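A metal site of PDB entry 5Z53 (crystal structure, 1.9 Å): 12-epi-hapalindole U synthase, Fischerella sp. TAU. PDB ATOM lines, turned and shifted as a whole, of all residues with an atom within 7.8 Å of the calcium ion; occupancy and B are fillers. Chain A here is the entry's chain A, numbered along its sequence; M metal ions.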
ATOM      1  N   PHE A  88      10.327  21.506  14.813  1.00  0.00           N
ATOM      2  CA  PHE A  88       8.945  21.702  14.444  1.00  0.00           C
ATOM      3  C   PHE A  88       8.388  23.101  14.746  1.00  0.00           C
ATOM      4  O   PHE A  88       7.214  23.371  14.465  1.00  0.00           O
ATOM      5  CB  PHE A  88       8.126  20.574  15.078  1.00  0.00           C
ATOM      6  CG  PHE A  88       8.675  19.199  14.762  1.00  0.00           C
ATOM      7  CD1 PHE A  88       8.776  18.740  13.452  1.00  0.00           C
ATOM      8  CD2 PHE A  88       9.132  18.360  15.771  1.00  0.00           C
ATOM      9  CE1 PHE A  88       9.298  17.490  13.163  1.00  0.00           C
ATOM     10  CE2 PHE A  88       9.625  17.096  15.480  1.00  0.00           C
ATOM     11  CZ  PHE A  88       9.747  16.673  14.167  1.00  0.00           C
ATOM     12  N   TYR A  89       9.220  24.026  15.234  1.00  0.00           N
ATOM     13  CA  TYR A  89       8.784  25.369  15.559  1.00  0.00           C
ATOM     14  C   TYR A  89       9.928  26.326  15.242  1.00  0.00           C
ATOM     15  O   TYR A  89      11.095  25.891  15.181  1.00  0.00           O
ATOM     16  CB  TYR A  89       8.438  25.486  17.062  1.00  0.00           C
ATOM     17  CG  TYR A  89       7.032  25.036  17.417  1.00  0.00           C
ATOM     18  CD1 TYR A  89       5.957  25.864  17.159  1.00  0.00           C
ATOM     19  CD2 TYR A  89       6.769  23.785  17.970  1.00  0.00           C
ATOM     20  CE1 TYR A  89       4.661  25.482  17.462  1.00  0.00           C
ATOM     21  CE2 TYR A  89       5.466  23.396  18.272  1.00  0.00           C
ATOM     22  CZ  TYR A  89       4.413  24.243  18.027  1.00  0.00           C
ATOM     23  OH  TYR A  89       3.108  23.910  18.269  1.00  0.00           O
ATOM     24  N   GLY A 136      -0.409  27.109  19.482  1.00  0.00           N
ATOM     25  CA  GLY A 136       0.724  26.778  18.656  1.00  0.00           C
ATOM     26  C   GLY A 136       0.344  25.909  17.485  1.00  0.00           C
ATOM     27  O   GLY A 136      -0.497  25.005  17.615  1.00  0.00           O
ATOM     28  N   ASN A 137       0.987  26.192  16.340  1.00  0.00           N
ATOM     29  CA  ASN A 137       0.802  25.453  15.096  1.00  0.00           C
ATOM     30  C   ASN A 137       2.089  24.717  14.709  1.00  0.00           C
ATOM     31  O   ASN A 137       2.997  25.341  14.127  1.00  0.00           O
ATOM     32  CB  ASN A 137       0.384  26.453  14.007  1.00  0.00           C
ATOM     33  CG  ASN A 137       0.179  25.840  12.647  1.00  0.00           C
ATOM     34  OD1 ASN A 137       0.373  24.644  12.486  1.00  0.00           O
ATOM     35  ND2 ASN A 137      -0.156  26.664  11.670  1.00  0.00           N
ATOM     36  N   LEU A 138       2.176  23.425  15.003  1.00  0.00           N
ATOM     37  CA  LEU A 138       3.326  22.518  14.678  1.00  0.00           C
ATOM     38  C   LEU A 138       3.651  22.637  13.195  1.00  0.00           C
ATOM     39  O   LEU A 138       2.731  22.622  12.372  1.00  0.00           O
ATOM     40  CB  LEU A 138       2.922  21.064  14.898  1.00  0.00           C
ATOM     41  CG  LEU A 138       3.667  20.150  15.878  1.00  0.00           C
ATOM     42  CD1 LEU A 138       3.772  18.776  15.264  1.00  0.00           C
ATOM     43  CD2 LEU A 138       5.044  20.610  16.326  1.00  0.00           C
ATOM     44  N   ALA A 139       4.946  22.690  12.874  1.00  0.00           N
ATOM     45  CA  ALA A 139       5.417  22.859  11.487  1.00  0.00           C
ATOM     46  C   ALA A 139       6.359  21.715  11.090  1.00  0.00           C
ATOM     47  O   ALA A 139       6.921  21.027  11.932  1.00  0.00           O
ATOM     48  CB  ALA A 139       6.107  24.182  11.330  1.00  0.00           C
ATOM     49  N   GLY A 140       6.487  21.531   9.776  1.00  0.00           N
ATOM     50  CA  GLY A 140       7.533  20.758   9.198  1.00  0.00           C
ATOM     51  C   GLY A 140       7.066  19.375   8.780  1.00  0.00           C
ATOM     52  O   GLY A 140       5.870  19.117   8.604  1.00  0.00           O
ATOM     53  N   SER A 146       3.510  14.744   7.581  1.00  0.00           N
ATOM     54  CA  SER A 146       3.531  16.176   7.342  1.00  0.00           C
ATOM     55  C   SER A 146       2.719  16.884   8.419  1.00  0.00           C
ATOM     56  O   SER A 146       1.548  16.531   8.651  1.00  0.00           O
ATOM     57  CB  SER A 146       3.005  16.555   5.983  1.00  0.00           C
ATOM     58  OG  SER A 146       2.871  17.971   5.922  1.00  0.00           O
ATOM     59  N   PHE A 147       3.305  17.956   8.939  1.00  0.00           N
ATOM     60  CA  PHE A 147       2.616  18.771   9.920  1.00  0.00           C
ATOM     61  C   PHE A 147       2.019  20.033   9.304  1.00  0.00           C
ATOM     62  O   PHE A 147       1.524  20.908  10.034  1.00  0.00           O
ATOM     63  CB  PHE A 147       3.568  19.149  11.034  1.00  0.00           C
ATOM     64  CG  PHE A 147       4.051  17.973  11.826  1.00  0.00           C
ATOM     65  CD1 PHE A 147       3.180  16.982  12.227  1.00  0.00           C
ATOM     66  CD2 PHE A 147       5.390  17.869  12.176  1.00  0.00           C
ATOM     67  CE1 PHE A 147       3.613  15.932  13.007  1.00  0.00           C
ATOM     68  CE2 PHE A 147       5.830  16.799  12.942  1.00  0.00           C
ATOM     69  CZ  PHE A 147       4.944  15.834  13.358  1.00  0.00           C
ATOM     70  N   ALA A 148       2.061  20.126   7.981  1.00  0.00           N
ATOM     71  CA  ALA A 148       1.448  21.259   7.298  1.00  0.00           C
ATOM     72  C   ALA A 148      -0.045  21.348   7.637  1.00  0.00           C
ATOM     73  O   ALA A 148      -0.761  20.341   7.700  1.00  0.00           O
ATOM     74  CB  ALA A 148       1.667  21.142   5.800  1.00  0.00           C
ATOM     75  N   GLY A 149      -0.505  22.570   7.887  1.00  0.00           N
ATOM     76  CA  GLY A 149      -1.910  22.841   8.149  1.00  0.00           C
ATOM     77  C   GLY A 149      -2.207  22.895   9.637  1.00  0.00           C
ATOM     78  O   GLY A 149      -1.357  22.648  10.468  1.00  0.00           O
ATOM     79  N   PHE A 150      -3.481  23.049   9.971  1.00  0.00           N
ATOM     80  CA  PHE A 150      -3.913  23.425  11.308  1.00  0.00           C
ATOM     81  C   PHE A 150      -5.407  23.115  11.450  1.00  0.00           C
ATOM     82  O   PHE A 150      -6.197  23.342  10.541  1.00  0.00           O
ATOM     83  CB  PHE A 150      -3.589  24.898  11.546  1.00  0.00           C
ATOM     84  CG  PHE A 150      -3.834  25.402  12.954  1.00  0.00           C
ATOM     85  CD1 PHE A 150      -2.919  25.144  13.974  1.00  0.00           C
ATOM     86  CD2 PHE A 150      -4.887  26.267  13.204  1.00  0.00           C
ATOM     87  CE1 PHE A 150      -3.114  25.693  15.236  1.00  0.00           C
ATOM     88  CE2 PHE A 150      -5.096  26.785  14.480  1.00  0.00           C
ATOM     89  CZ  PHE A 150      -4.202  26.491  15.494  1.00  0.00           C
ATOM     90  N   PRO A 151      -5.831  22.523  12.581  1.00  0.00           N
ATOM     91  CA  PRO A 151      -7.224  22.120  12.750  1.00  0.00           C
ATOM     92  C   PRO A 151      -8.220  23.211  13.190  1.00  0.00           C
ATOM     93  O   PRO A 151      -9.436  22.970  13.202  1.00  0.00           O
ATOM     94  CB  PRO A 151      -7.110  21.054  13.849  1.00  0.00           C
ATOM     95  CG  PRO A 151      -5.971  21.517  14.696  1.00  0.00           C
ATOM     96  CD  PRO A 151      -4.988  22.129  13.729  1.00  0.00           C
ATOM     97  N   ILE A 173      -2.493  31.684  12.954  1.00  0.00           N
ATOM     98  CA  ILE A 173      -1.284  31.196  13.544  1.00  0.00           C
ATOM     99  C   ILE A 173      -0.459  30.533  12.456  1.00  0.00           C
ATOM    100  O   ILE A 173      -0.871  29.529  11.851  1.00  0.00           O
ATOM    101  CB  ILE A 173      -1.600  30.243  14.706  1.00  0.00           C
ATOM    102  CG1 ILE A 173      -2.602  30.927  15.632  1.00  0.00           C
ATOM    103  CG2 ILE A 173      -0.309  29.843  15.393  1.00  0.00           C
ATOM    104  CD1 ILE A 173      -3.119  30.077  16.722  1.00  0.00           C
ATOM    105  N   LYS A 174       0.668  31.167  12.194  1.00  0.00           N
ATOM    106  CA  LYS A 174       1.590  30.691  11.213  1.00  0.00           C
ATOM    107  C   LYS A 174       2.193  29.360  11.671  1.00  0.00           C
ATOM    108  O   LYS A 174       2.367  29.094  12.886  1.00  0.00           O
ATOM    109  CB  LYS A 174       2.747  31.667  11.043  1.00  0.00           C
ATOM    110  CG  LYS A 174       2.433  32.915  10.248  1.00  0.00           C
ATOM    111  CD  LYS A 174       3.681  33.752  10.014  1.00  0.00           C
ATOM    112  CE  LYS A 174       3.489  34.781   8.921  1.00  0.00           C
ATOM    113  NZ  LYS A 174       3.164  36.096   9.512  1.00  0.00           N
ATOM    114  N   GLU A 175       2.563  28.576  10.659  1.00  0.00           N
ATOM    115  CA  GLU A 175       3.244  27.323  10.783  1.00  0.00           C
ATOM    116  C   GLU A 175       4.503  27.594  11.614  1.00  0.00           C
ATOM    117  O   GLU A 175       5.271  28.452  11.262  1.00  0.00           O
ATOM    118  CB  GLU A 175       3.540  26.732   9.406  1.00  0.00           C
ATOM    119  CG  GLU A 175       2.328  26.184   8.656  1.00  0.00           C
ATOM    120  CD  GLU A 175       1.762  24.893   9.235  1.00  0.00           C
ATOM    121  OE1 GLU A 175       2.566  24.007   9.605  1.00  0.00           O
ATOM    122  OE2 GLU A 175       0.536  24.772   9.365  1.00  0.00           O
ATOM    123  N   GLY A 176       4.618  26.938  12.759  1.00  0.00           N
ATOM    124  CA  GLY A 176       5.841  26.992  13.556  1.00  0.00           C
ATOM    125  C   GLY A 176       5.887  28.149  14.538  1.00  0.00           C
ATOM    126  O   GLY A 176       6.937  28.375  15.113  1.00  0.00           O
ATOM    127  N   LYS A 209      -6.616  19.356   8.595  1.00  0.00           N
ATOM    128  CA  LYS A 209      -5.340  18.816   9.089  1.00  0.00           C
ATOM    129  C   LYS A 209      -4.154  19.490   8.403  1.00  0.00           C
ATOM    130  O   LYS A 209      -4.324  20.270   7.461  1.00  0.00           O
ATOM    131  CB  LYS A 209      -5.244  17.303   8.927  1.00  0.00           C
ATOM    132  CG  LYS A 209      -6.178  16.688   7.905  1.00  0.00           C
ATOM    133  CD  LYS A 209      -5.672  16.894   6.515  1.00  0.00           C
ATOM    134  CE  LYS A 209      -6.169  15.816   5.580  1.00  0.00           C
ATOM    135  NZ  LYS A 209      -5.756  16.104   4.180  1.00  0.00           N
ATOM    136  N   PHE A 210      -2.943  19.189   8.900  1.00  0.00           N
ATOM    137  CA  PHE A 210      -2.628  18.419  10.094  1.00  0.00           C
ATOM    138  C   PHE A 210      -3.467  18.813  11.330  1.00  0.00           C
ATOM    139  O   PHE A 210      -3.642  20.009  11.623  1.00  0.00           O
ATOM    140  CB  PHE A 210      -1.129  18.594  10.383  1.00  0.00           C
ATOM    141  CG  PHE A 210      -0.655  18.021  11.673  1.00  0.00           C
ATOM    142  CD1 PHE A 210      -0.525  16.654  11.806  1.00  0.00           C
ATOM    143  CD2 PHE A 210      -0.384  18.844  12.758  1.00  0.00           C
ATOM    144  CE1 PHE A 210      -0.097  16.101  13.000  1.00  0.00           C
ATOM    145  CE2 PHE A 210      -0.012  18.287  13.974  1.00  0.00           C
ATOM    146  CZ  PHE A 210       0.138  16.917  14.085  1.00  0.00           C
ATOM    147  N   SER A 211      -3.994  17.807  12.029  1.00  0.00           N
ATOM    148  CA  SER A 211      -5.055  18.018  13.041  1.00  0.00           C
ATOM    149  C   SER A 211      -4.525  17.810  14.478  1.00  0.00           C
ATOM    150  O   SER A 211      -5.215  17.301  15.362  1.00  0.00           O
ATOM    151  CB  SER A 211      -6.305  17.191  12.715  1.00  0.00           C
ATOM    152  OG  SER A 211      -6.063  15.815  12.821  1.00  0.00           O
ATOM    153  N   GLY A 212      -3.319  18.316  14.748  1.00  0.00           N
ATOM    154  CA  GLY A 212      -2.858  18.536  16.115  1.00  0.00           C
ATOM    155  C   GLY A 212      -2.673  20.029  16.395  1.00  0.00           C
ATOM    156  O   GLY A 212      -2.531  20.845  15.478  1.00  0.00           O
HETATM  157 CA    CA M   1       0.907  22.958  10.948  1.00  0.00          CA
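OG of Ser 146 is in hydrogen-bond range of N of Ala 148, 3.1 Å away. The side-chain hydroxyl of Tyr 89 lies within hydrogen-bond range of the backbone NH of Leu 138, 3.4 Å away. The backbone carbonyl oxygen (O) of Asn 137 sits at hydrogen-bond distance from the backbone NH (N) of Gly 176 (2.7 Å). The backbone carbonyl oxygen (O) of Gly 140 is in hydrogen-bond range of the backbone NH (N) of Phe 147. O of Ala 148 lies within hydrogen-bond range of N of Phe 210 (2.7 Å). ND2 of Asn 137 is in hydrogen-bond range of O of Ile 173 (3.0 Å).
Residues that only touch the calcium ion: Ala 148. Of the 21 residues printed, 6 come within 4 Å of the calcium ion. The nearest printed residue that does not touch the calcium ion is Ala 139 (4.5 Å).
The calcium ion is bound by O of Phe 147 (2.3 Å), O of Gly 149 (2.3 Å), O of Leu 138 (2.3 Å), OD1 of Asn 137 (2.3 Å), OE1 of Glu 175 (2.4 Å) and OE2 of Glu 175 (2.4 Å).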
